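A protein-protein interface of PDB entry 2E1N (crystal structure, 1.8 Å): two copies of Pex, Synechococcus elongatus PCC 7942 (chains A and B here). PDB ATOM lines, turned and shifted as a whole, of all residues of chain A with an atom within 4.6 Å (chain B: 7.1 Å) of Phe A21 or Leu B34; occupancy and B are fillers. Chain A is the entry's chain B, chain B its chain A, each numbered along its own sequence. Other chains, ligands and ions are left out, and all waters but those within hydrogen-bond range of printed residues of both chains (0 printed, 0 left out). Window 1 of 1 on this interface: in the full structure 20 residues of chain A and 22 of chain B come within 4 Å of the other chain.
The backbone NH (N) of Leu B34 sits at hydrogen-bond distance from the side-chain hydroxyl (OG) of Ser B31 (3.3 Å). The side-chain carboxylate (OE2) of Glu B33 lies within salt-bridge range of the side-chain amino group (NZ) of Lys B32 (2.9 Å). The side-chain sulfur (SG) of Cys B37 lies within hydrogen-bond range of the backbone carbonyl oxygen (O) of Glu B33, at 3.6 Å. The side-chain hydroxyl of Ser B31 sits at hydrogen-bond distance from the side-chain carboxylate of Glu B33 (3.2 Å). The backbone carbonyl oxygen of Leu B114 sits close to the side-chain sulfur of Cys B37, at 3.5 Å.
CG2 of Ile A18 touches SG of Cys B37 (3.9 Å). CG2 of Ile A18 touches CD2 of Leu B114, at 3.8 Å. CE2 of Tyr A19 touches CD1 of Leu B117, at 3.9 Å. Phe A21 touches Ser B31. OE1 of Glu B33 touches CD1 of Phe A21, 3.6 Å away. Phe A21 touches Leu B34 (CE2 to CD1, 3.4 Å). Leu B34 touches Phe A22 (CD1 to CZ, 3.2 Å). SG of Cys B37 touches CE1 of Phe A22, at 3.5 Å. Phe A22 touches Leu B117 (CE2 to O, 3.5 Å). Tyr B121 touches Phe A22.
Printed residues of chain B within 4 Å of Ile A18: Val B36 (3.9 Å), Cys B37 (3.9 Å) and Leu B114 (3.8 Å). Printed residues of chain B within 4 Å of Phe A21: Ser B31 (3.3 Å), Glu B33 (3.6 Å) and Leu B34 (3.4 Å). Printed residues of chain B within 4 Å of Phe A22: Leu B34 (3.2 Å), Cys B37 (3.5 Å), Leu B117 (3.5 Å) and Tyr B121 (3.9 Å). Printed residues of chain A within 4 Å of Cys B37: Ile A18 and Phe A22. Of the printed residues of chain A, Leu B114 touches Ile A18 (3.8 Å).
Hydrophobic or aromatic side chains of chain A that line the printed part of chain B: Ile A18, Tyr A19, Phe A21 and Phe A22. Of the 20 printed residues of chain B, 8 touch a printed residue of chain A. Among the printed residues, 11 pairs touch across the chains. Among the printed residues, no Asp or Glu carboxylate lies within 4 Å of a Lys or Arg side-chain nitrogen of the other chain.
No position is printed for both chains. Of the 11 pairs that touch across the chains among the printed residues, none has its exchanged pair printed and touching as well.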
ATOM      1  N   ASP A  17     -20.369   1.776  31.504  1.00  0.00           N
ATOM      2  CA  ASP A  17     -19.236   2.583  31.022  1.00  0.00           C
ATOM      3  C   ASP A  17     -19.267   2.675  29.508  1.00  0.00           C
ATOM      4  O   ASP A  17     -19.113   3.763  28.938  1.00  0.00           O
ATOM      5  CB  ASP A  17     -17.882   2.000  31.431  1.00  0.00           C
ATOM      6  CG  ASP A  17     -17.719   1.896  32.929  1.00  0.00           C
ATOM      7  OD1 ASP A  17     -18.170   2.824  33.644  1.00  0.00           O
ATOM      8  OD2 ASP A  17     -17.149   0.878  33.399  1.00  0.00           O
ATOM      9  N   ILE A  18     -19.474   1.531  28.868  1.00  0.00           N
ATOM     10  CA  ILE A  18     -19.393   1.453  27.424  1.00  0.00           C
ATOM     11  C   ILE A  18     -20.453   2.368  26.799  1.00  0.00           C
ATOM     12  O   ILE A  18     -20.119   3.270  26.061  1.00  0.00           O
ATOM     13  CB  ILE A  18     -19.482  -0.008  26.907  1.00  0.00           C
ATOM     14  CG1 ILE A  18     -18.246  -0.789  27.374  1.00  0.00           C
ATOM     15  CG2 ILE A  18     -19.555  -0.039  25.382  1.00  0.00           C
ATOM     16  CD1 ILE A  18     -18.323  -2.278  27.099  1.00  0.00           C
ATOM     17  N   TYR A  19     -21.718   2.166  27.135  1.00  0.00           N
ATOM     18  CA  TYR A  19     -22.785   3.009  26.549  1.00  0.00           C
ATOM     19  C   TYR A  19     -22.603   4.490  26.905  1.00  0.00           C
ATOM     20  O   TYR A  19     -22.766   5.364  26.055  1.00  0.00           O
ATOM     21  CB  TYR A  19     -24.178   2.507  26.952  1.00  0.00           C
ATOM     22  CG  TYR A  19     -24.591   1.273  26.185  1.00  0.00           C
ATOM     23  CD1 TYR A  19     -24.244   0.003  26.630  1.00  0.00           C
ATOM     24  CD2 TYR A  19     -25.304   1.383  24.992  1.00  0.00           C
ATOM     25  CE1 TYR A  19     -24.610  -1.120  25.927  1.00  0.00           C
ATOM     26  CE2 TYR A  19     -25.673   0.258  24.271  1.00  0.00           C
ATOM     27  CZ  TYR A  19     -25.317  -0.988  24.744  1.00  0.00           C
ATOM     28  OH  TYR A  19     -25.673  -2.088  24.025  1.00  0.00           O
ATOM     29  N   ARG A  20     -22.251   4.754  28.160  1.00  0.00           N
ATOM     30  CA  ARG A  20     -21.961   6.105  28.634  1.00  0.00           C
ATOM     31  C   ARG A  20     -20.828   6.760  27.860  1.00  0.00           C
ATOM     32  O   ARG A  20     -20.884   7.951  27.569  1.00  0.00           O
ATOM     33  CB  ARG A  20     -21.575   6.051  30.099  1.00  0.00           C
ATOM     34  CG  ARG A  20     -21.530   7.394  30.811  1.00  0.00           C
ATOM     35  CD  ARG A  20     -21.661   7.159  32.328  1.00  0.00           C
ATOM     36  NE  ARG A  20     -20.631   6.225  32.803  1.00  0.00           N
ATOM     37  CZ  ARG A  20     -20.581   5.691  34.022  1.00  0.00           C
ATOM     38  NH1 ARG A  20     -21.510   5.966  34.935  1.00  0.00           N
ATOM     39  NH2 ARG A  20     -19.583   4.864  34.322  1.00  0.00           N
ATOM     40  N   PHE A  21     -19.783   5.987  27.546  1.00  0.00           N
ATOM     41  CA  PHE A  21     -18.716   6.490  26.682  1.00  0.00           C
ATOM     42  C   PHE A  21     -19.274   6.919  25.329  1.00  0.00           C
ATOM     43  O   PHE A  21     -18.906   7.983  24.800  1.00  0.00           O
ATOM     44  CB  PHE A  21     -17.611   5.449  26.457  1.00  0.00           C
ATOM     45  CG  PHE A  21     -16.480   5.949  25.591  1.00  0.00           C
ATOM     46  CD1 PHE A  21     -15.376   6.563  26.153  1.00  0.00           C
ATOM     47  CD2 PHE A  21     -16.538   5.822  24.207  1.00  0.00           C
ATOM     48  CE1 PHE A  21     -14.330   7.029  25.352  1.00  0.00           C
ATOM     49  CE2 PHE A  21     -15.511   6.307  23.392  1.00  0.00           C
ATOM     50  CZ  PHE A  21     -14.393   6.906  23.979  1.00  0.00           C
ATOM     51  N   PHE A  22     -20.141   6.099  24.746  1.00  0.00           N
ATOM     52  CA  PHE A  22     -20.610   6.410  23.394  1.00  0.00           C
ATOM     53  C   PHE A  22     -21.633   7.540  23.405  1.00  0.00           C
ATOM     54  O   PHE A  22     -21.801   8.235  22.410  1.00  0.00           O
ATOM     55  CB  PHE A  22     -21.174   5.167  22.697  1.00  0.00           C
ATOM     56  CG  PHE A  22     -20.122   4.255  22.191  1.00  0.00           C
ATOM     57  CD1 PHE A  22     -19.658   3.216  22.971  1.00  0.00           C
ATOM     58  CD2 PHE A  22     -19.559   4.454  20.944  1.00  0.00           C
ATOM     59  CE1 PHE A  22     -18.661   2.366  22.504  1.00  0.00           C
ATOM     60  CE2 PHE A  22     -18.571   3.612  20.474  1.00  0.00           C
ATOM     61  CZ  PHE A  22     -18.131   2.556  21.262  1.00  0.00           C
ATOM     62  N   GLN A  23     -22.323   7.707  24.523  1.00  0.00           N
ATOM     63  CA  GLN A  23     -23.323   8.759  24.639  1.00  0.00           C
ATOM     64  C   GLN A  23     -22.632  10.108  24.784  1.00  0.00           C
ATOM     65  O   GLN A  23     -23.024  11.090  24.137  1.00  0.00           O
ATOM     66  CB  GLN A  23     -24.191   8.532  25.863  1.00  0.00           C
ATOM     67  CG  GLN A  23     -25.267   9.612  26.074  1.00  0.00           C
ATOM     68  CD  GLN A  23     -25.773   9.661  27.507  1.00  0.00           C
ATOM     69  OE1 GLN A  23     -25.532   8.737  28.296  1.00  0.00           O
ATOM     70  NE2 GLN A  23     -26.499  10.743  27.849  1.00  0.00           N
ATOM     71  N   ASP A  24     -21.620  10.149  25.645  1.00  0.00           N
ATOM     72  CA  ASP A  24     -20.923  11.404  26.014  1.00  0.00           C
ATOM     73  C   ASP A  24     -19.454  11.150  26.206  1.00  0.00           C
ATOM     74  O   ASP A  24     -19.027  11.070  27.350  1.00  0.00           O
ATOM     75  CB  ASP A  24     -21.401  11.865  27.398  1.00  0.00           C
ATOM     76  CG  ASP A  24     -22.738  12.539  27.382  1.00  0.00           C
ATOM     77  OD1 ASP A  24     -22.755  13.776  27.143  1.00  0.00           O
ATOM     78  OD2 ASP A  24     -23.752  11.845  27.677  1.00  0.00           O
ATOM     79  N   PRO A  25     -18.676  10.972  25.128  1.00  0.00           N
ATOM     80  CA  PRO A  25     -17.230  10.741  25.363  1.00  0.00           C
ATOM     81  C   PRO A  25     -16.525  11.974  25.926  1.00  0.00           C
ATOM     82  O   PRO A  25     -17.074  13.084  25.846  1.00  0.00           O
ATOM     83  CB  PRO A  25     -16.691  10.360  23.968  1.00  0.00           C
ATOM     84  CG  PRO A  25     -17.706  10.866  23.020  1.00  0.00           C
ATOM     85  CD  PRO A  25     -19.030  10.910  23.707  1.00  0.00           C
ATOM     86  N   PRO A  26     -15.326  11.803  26.505  1.00  0.00           N
ATOM     87  CA  PRO A  26     -14.608  12.991  26.914  1.00  0.00           C
ATOM     88  C   PRO A  26     -14.347  13.866  25.687  1.00  0.00           C
ATOM     89  O   PRO A  26     -14.121  13.330  24.587  1.00  0.00           O
ATOM     90  CB  PRO A  26     -13.298  12.438  27.502  1.00  0.00           C
ATOM     91  CG  PRO A  26     -13.560  11.037  27.808  1.00  0.00           C
ATOM     92  CD  PRO A  26     -14.600  10.569  26.842  1.00  0.00           C
ATOM     93  N   TYR B  29      -5.386   6.807  19.438  1.00  0.00           N
ATOM     94  CA  TYR B  29      -5.490   5.464  20.069  1.00  0.00           C
ATOM     95  C   TYR B  29      -6.887   5.216  20.658  1.00  0.00           C
ATOM     96  O   TYR B  29      -7.469   6.076  21.344  1.00  0.00           O
ATOM     97  CB  TYR B  29      -4.451   5.257  21.178  1.00  0.00           C
ATOM     98  CG  TYR B  29      -3.096   4.893  20.653  1.00  0.00           C
ATOM     99  CD1 TYR B  29      -2.175   5.872  20.310  1.00  0.00           C
ATOM    100  CD2 TYR B  29      -2.734   3.566  20.462  1.00  0.00           C
ATOM    101  CE1 TYR B  29      -0.919   5.536  19.789  1.00  0.00           C
ATOM    102  CE2 TYR B  29      -1.488   3.227  19.957  1.00  0.00           C
ATOM    103  CZ  TYR B  29      -0.595   4.206  19.611  1.00  0.00           C
ATOM    104  OH  TYR B  29       0.644   3.864  19.129  1.00  0.00           O
ATOM    105  N   LEU B  30      -7.406   4.009  20.465  1.00  0.00           N
ATOM    106  CA  LEU B  30      -8.709   3.643  21.025  1.00  0.00           C
ATOM    107  C   LEU B  30      -8.687   3.582  22.515  1.00  0.00           C
ATOM    108  O   LEU B  30      -7.709   3.108  23.132  1.00  0.00           O
ATOM    109  CB  LEU B  30      -9.112   2.264  20.482  1.00  0.00           C
ATOM    110  CG  LEU B  30      -9.293   2.050  18.991  1.00  0.00           C
ATOM    111  CD1 LEU B  30      -9.959   0.681  18.721  1.00  0.00           C
ATOM    112  CD2 LEU B  30     -10.133   3.176  18.406  1.00  0.00           C
ATOM    113  N   SER B  31      -9.783   4.037  23.129  1.00  0.00           N
ATOM    114  CA  SER B  31     -10.031   3.762  24.540  1.00  0.00           C
ATOM    115  C   SER B  31     -10.465   2.344  24.740  1.00  0.00           C
ATOM    116  O   SER B  31     -10.827   1.660  23.790  1.00  0.00           O
ATOM    117  CB  SER B  31     -11.122   4.687  25.075  1.00  0.00           C
ATOM    118  OG  SER B  31     -12.338   4.377  24.435  1.00  0.00           O
ATOM    119  N   LYS B  32     -10.471   1.890  25.985  1.00  0.00           N
ATOM    120  CA  LYS B  32     -10.917   0.534  26.277  1.00  0.00           C
ATOM    121  C   LYS B  32     -12.351   0.305  25.816  1.00  0.00           C
ATOM    122  O   LYS B  32     -12.692  -0.758  25.353  1.00  0.00           O
ATOM    123  CB  LYS B  32     -10.748   0.200  27.770  1.00  0.00           C
ATOM    124  CG  LYS B  32     -11.530   1.035  28.728  1.00  0.00           C
ATOM    125  CD  LYS B  32     -11.123   0.649  30.185  1.00  0.00           C
ATOM    126  CE  LYS B  32     -12.040   1.274  31.214  1.00  0.00           C
ATOM    127  NZ  LYS B  32     -12.183   2.744  31.072  1.00  0.00           N
ATOM    128  N   GLU B  33     -13.209   1.317  25.935  1.00  0.00           N
ATOM    129  CA  GLU B  33     -14.598   1.130  25.515  1.00  0.00           C
ATOM    130  C   GLU B  33     -14.706   0.949  24.003  1.00  0.00           C
ATOM    131  O   GLU B  33     -15.419   0.073  23.515  1.00  0.00           O
ATOM    132  CB  GLU B  33     -15.445   2.327  25.947  1.00  0.00           C
ATOM    133  CG  GLU B  33     -15.505   2.486  27.478  1.00  0.00           C
ATOM    134  CD  GLU B  33     -14.372   3.353  28.103  1.00  0.00           C
ATOM    135  OE1 GLU B  33     -13.414   3.805  27.408  1.00  0.00           O
ATOM    136  OE2 GLU B  33     -14.428   3.543  29.339  1.00  0.00           O
ATOM    137  N   LEU B  34     -14.011   1.796  23.258  1.00  0.00           N
ATOM    138  CA  LEU B  34     -13.969   1.634  21.806  1.00  0.00           C
ATOM    139  C   LEU B  34     -13.321   0.306  21.415  1.00  0.00           C
ATOM    140  O   LEU B  34     -13.769  -0.327  20.465  1.00  0.00           O
ATOM    141  CB  LEU B  34     -13.217   2.806  21.145  1.00  0.00           C
ATOM    142  CG  LEU B  34     -13.936   3.935  20.419  1.00  0.00           C
ATOM    143  CD1 LEU B  34     -15.357   4.044  20.803  1.00  0.00           C
ATOM    144  CD2 LEU B  34     -13.128   5.281  20.565  1.00  0.00           C
ATOM    145  N   ALA B  35     -12.256  -0.082  22.106  1.00  0.00           N
ATOM    146  CA  ALA B  35     -11.540  -1.321  21.785  1.00  0.00           C
ATOM    147  C   ALA B  35     -12.446  -2.515  21.909  1.00  0.00           C
ATOM    148  O   ALA B  35     -12.390  -3.434  21.098  1.00  0.00           O
ATOM    149  CB  ALA B  35     -10.317  -1.500  22.675  1.00  0.00           C
ATOM    150  N   VAL B  36     -13.274  -2.548  22.938  1.00  0.00           N
ATOM    151  CA  VAL B  36     -14.217  -3.678  23.146  1.00  0.00           C
ATOM    152  C   VAL B  36     -15.122  -3.822  21.953  1.00  0.00           C
ATOM    153  O   VAL B  36     -15.300  -4.936  21.413  1.00  0.00           O
ATOM    154  CB  VAL B  36     -15.010  -3.481  24.474  1.00  0.00           C
ATOM    155  CG1 VAL B  36     -16.291  -4.344  24.541  1.00  0.00           C
ATOM    156  CG2 VAL B  36     -14.066  -3.727  25.668  1.00  0.00           C
ATOM    157  N   CYS B  37     -15.687  -2.685  21.496  1.00  0.00           N
ATOM    158  CA  CYS B  37     -16.639  -2.698  20.385  1.00  0.00           C
ATOM    159  C   CYS B  37     -15.943  -3.013  19.069  1.00  0.00           C
ATOM    160  O   CYS B  37     -16.492  -3.722  18.262  1.00  0.00           O
ATOM    161  CB  CYS B  37     -17.344  -1.363  20.298  1.00  0.00           C
ATOM    162  SG  CYS B  37     -18.356  -1.078  21.827  1.00  0.00           S
ATOM    163  N   TYR B  38     -14.739  -2.489  18.861  1.00  0.00           N
ATOM    164  CA  TYR B  38     -13.957  -2.872  17.672  1.00  0.00           C
ATOM    165  C   TYR B  38     -13.671  -4.366  17.600  1.00  0.00           C
ATOM    166  O   TYR B  38     -13.830  -5.020  16.564  1.00  0.00           O
ATOM    167  CB  TYR B  38     -12.639  -2.066  17.653  1.00  0.00           C
ATOM    168  CG  TYR B  38     -11.601  -2.628  16.749  1.00  0.00           C
ATOM    169  CD1 TYR B  38     -11.829  -2.767  15.391  1.00  0.00           C
ATOM    170  CD2 TYR B  38     -10.406  -3.103  17.254  1.00  0.00           C
ATOM    171  CE1 TYR B  38     -10.901  -3.331  14.570  1.00  0.00           C
ATOM    172  CE2 TYR B  38      -9.477  -3.695  16.420  1.00  0.00           C
ATOM    173  CZ  TYR B  38      -9.744  -3.822  15.079  1.00  0.00           C
ATOM    174  OH  TYR B  38      -8.813  -4.454  14.247  1.00  0.00           O
ATOM    175  N   VAL B  39     -13.169  -4.901  18.699  1.00  0.00           N
ATOM    176  CA  VAL B  39     -12.794  -6.311  18.741  1.00  0.00           C
ATOM    177  C   VAL B  39     -14.004  -7.191  18.428  1.00  0.00           C
ATOM    178  O   VAL B  39     -13.932  -8.146  17.621  1.00  0.00           O
ATOM    179  CB  VAL B  39     -12.196  -6.681  20.100  1.00  0.00           C
ATOM    180  CG1 VAL B  39     -12.111  -8.223  20.212  1.00  0.00           C
ATOM    181  CG2 VAL B  39     -10.772  -6.067  20.293  1.00  0.00           C
ATOM    182  N   LEU B  40     -15.144  -6.858  19.015  1.00  0.00           N
ATOM    183  CA  LEU B  40     -16.370  -7.581  18.729  1.00  0.00           C
ATOM    184  C   LEU B  40     -16.806  -7.453  17.264  1.00  0.00           C
ATOM    185  O   LEU B  40     -17.227  -8.446  16.672  1.00  0.00           O
ATOM    186  CB  LEU B  40     -17.483  -7.163  19.687  1.00  0.00           C
ATOM    187  CG  LEU B  40     -17.308  -7.594  21.134  1.00  0.00           C
ATOM    188  CD1 LEU B  40     -18.453  -7.091  22.016  1.00  0.00           C
ATOM    189  CD2 LEU B  40     -17.198  -9.129  21.168  1.00  0.00           C
ATOM    190  N   TYR B  64      -7.115   5.335  13.371  1.00  0.00           N
ATOM    191  CA  TYR B  64      -7.066   4.792  14.745  1.00  0.00           C
ATOM    192  C   TYR B  64      -5.917   3.794  14.930  1.00  0.00           C
ATOM    193  O   TYR B  64      -5.440   3.191  13.985  1.00  0.00           O
ATOM    194  CB  TYR B  64      -8.379   4.080  15.106  1.00  0.00           C
ATOM    195  CG  TYR B  64      -9.539   5.035  15.025  1.00  0.00           C
ATOM    196  CD1 TYR B  64      -9.811   5.924  16.046  1.00  0.00           C
ATOM    197  CD2 TYR B  64     -10.308   5.106  13.880  1.00  0.00           C
ATOM    198  CE1 TYR B  64     -10.877   6.837  15.938  1.00  0.00           C
ATOM    199  CE2 TYR B  64     -11.376   6.026  13.774  1.00  0.00           C
ATOM    200  CZ  TYR B  64     -11.644   6.866  14.801  1.00  0.00           C
ATOM    201  OH  TYR B  64     -12.699   7.785  14.656  1.00  0.00           O
ATOM    202  N   LEU B  66      -4.333   0.885  18.180  1.00  0.00           N
ATOM    203  CA  LEU B  66      -4.647   0.120  19.359  1.00  0.00           C
ATOM    204  C   LEU B  66      -3.357  -0.381  19.980  1.00  0.00           C
ATOM    205  O   LEU B  66      -2.500  -0.982  19.281  1.00  0.00           O
ATOM    206  CB  LEU B  66      -5.576  -1.054  19.012  1.00  0.00           C
ATOM    207  CG  LEU B  66      -5.986  -1.996  20.135  1.00  0.00           C
ATOM    208  CD1 LEU B  66      -6.841  -1.259  21.190  1.00  0.00           C
ATOM    209  CD2 LEU B  66      -6.753  -3.208  19.449  1.00  0.00           C
ATOM    210  N   VAL B  70      -4.321  -1.625  25.982  1.00  0.00           N
ATOM    211  CA  VAL B  70      -5.763  -1.480  25.835  1.00  0.00           C
ATOM    212  C   VAL B  70      -6.368  -2.739  25.271  1.00  0.00           C
ATOM    213  O   VAL B  70      -7.453  -3.145  25.698  1.00  0.00           O
ATOM    214  CB  VAL B  70      -6.080  -0.223  25.001  1.00  0.00           C
ATOM    215  CG1 VAL B  70      -7.566  -0.109  24.638  1.00  0.00           C
ATOM    216  CG2 VAL B  70      -5.628   1.054  25.809  1.00  0.00           C
ATOM    217  N   ALA B  74      -9.462  -4.902  26.988  1.00  0.00           N
ATOM    218  CA  ALA B  74     -10.683  -5.239  26.254  1.00  0.00           C
ATOM    219  C   ALA B  74     -10.876  -6.732  26.219  1.00  0.00           C
ATOM    220  O   ALA B  74     -11.985  -7.204  26.494  1.00  0.00           O
ATOM    221  CB  ALA B  74     -10.638  -4.655  24.810  1.00  0.00           C
ATOM    222  N   LEU B 114     -22.982  -4.050  20.527  1.00  0.00           N
ATOM    223  CA  LEU B 114     -21.697  -3.421  20.792  1.00  0.00           C
ATOM    224  C   LEU B 114     -20.952  -3.193  19.490  1.00  0.00           C
ATOM    225  O   LEU B 114     -20.431  -2.124  19.272  1.00  0.00           O
ATOM    226  CB  LEU B 114     -20.883  -4.263  21.758  1.00  0.00           C
ATOM    227  CG  LEU B 114     -21.452  -4.337  23.180  1.00  0.00           C
ATOM    228  CD1 LEU B 114     -20.631  -5.285  24.086  1.00  0.00           C
ATOM    229  CD2 LEU B 114     -21.513  -2.940  23.781  1.00  0.00           C
ATOM    230  N   LEU B 117     -22.208  -0.115  17.924  1.00  0.00           N
ATOM    231  CA  LEU B 117     -21.721   1.148  18.489  1.00  0.00           C
ATOM    232  C   LEU B 117     -20.425   1.582  17.753  1.00  0.00           C
ATOM    233  O   LEU B 117     -20.218   2.767  17.490  1.00  0.00           O
ATOM    234  CB  LEU B 117     -21.505   1.038  20.016  1.00  0.00           C
ATOM    235  CG  LEU B 117     -22.707   0.826  20.950  1.00  0.00           C
ATOM    236  CD1 LEU B 117     -22.274   0.562  22.397  1.00  0.00           C
ATOM    237  CD2 LEU B 117     -23.666   2.000  20.888  1.00  0.00           C
ATOM    238  N   TRP B 118     -19.561   0.620  17.424  1.00  0.00           N
ATOM    239  CA  TRP B 118     -18.325   0.882  16.663  1.00  0.00           C
ATOM    240  C   TRP B 118     -18.612   1.423  15.251  1.00  0.00           C
ATOM    241  O   TRP B 118     -18.103   2.461  14.853  1.00  0.00           O
ATOM    242  CB  TRP B 118     -17.480  -0.407  16.573  1.00  0.00           C
ATOM    243  CG  TRP B 118     -16.289  -0.353  15.695  1.00  0.00           C
ATOM    244  CD1 TRP B 118     -16.100  -1.057  14.565  1.00  0.00           C
ATOM    245  CD2 TRP B 118     -15.096   0.444  15.869  1.00  0.00           C
ATOM    246  NE1 TRP B 118     -14.890  -0.758  13.999  1.00  0.00           N
ATOM    247  CE2 TRP B 118     -14.249   0.167  14.779  1.00  0.00           C
ATOM    248  CE3 TRP B 118     -14.675   1.353  16.830  1.00  0.00           C
ATOM    249  CZ2 TRP B 118     -12.994   0.769  14.626  1.00  0.00           C
ATOM    250  CZ3 TRP B 118     -13.423   1.957  16.675  1.00  0.00           C
ATOM    251  CH2 TRP B 118     -12.600   1.655  15.581  1.00  0.00           C
ATOM    252  N   TYR B 121     -20.006   4.850  15.597  1.00  0.00           N
ATOM    253  CA  TYR B 121     -18.952   5.780  15.983  1.00  0.00           C
ATOM    254  C   TYR B 121     -18.173   6.227  14.770  1.00  0.00           C
ATOM    255  O   TYR B 121     -17.791   7.386  14.685  1.00  0.00           O
ATOM    256  CB  TYR B 121     -17.964   5.128  16.947  1.00  0.00           C
ATOM    257  CG  TYR B 121     -16.901   6.051  17.498  1.00  0.00           C
ATOM    258  CD1 TYR B 121     -15.613   6.084  16.955  1.00  0.00           C
ATOM    259  CD2 TYR B 121     -17.173   6.867  18.573  1.00  0.00           C
ATOM    260  CE1 TYR B 121     -14.650   6.930  17.476  1.00  0.00           C
ATOM    261  CE2 TYR B 121     -16.221   7.694  19.097  1.00  0.00           C
ATOM    262  CZ  TYR B 121     -14.961   7.725  18.552  1.00  0.00           C
ATOM    263  OH  TYR B 121     -14.039   8.577  19.105  1.00  0.00           O
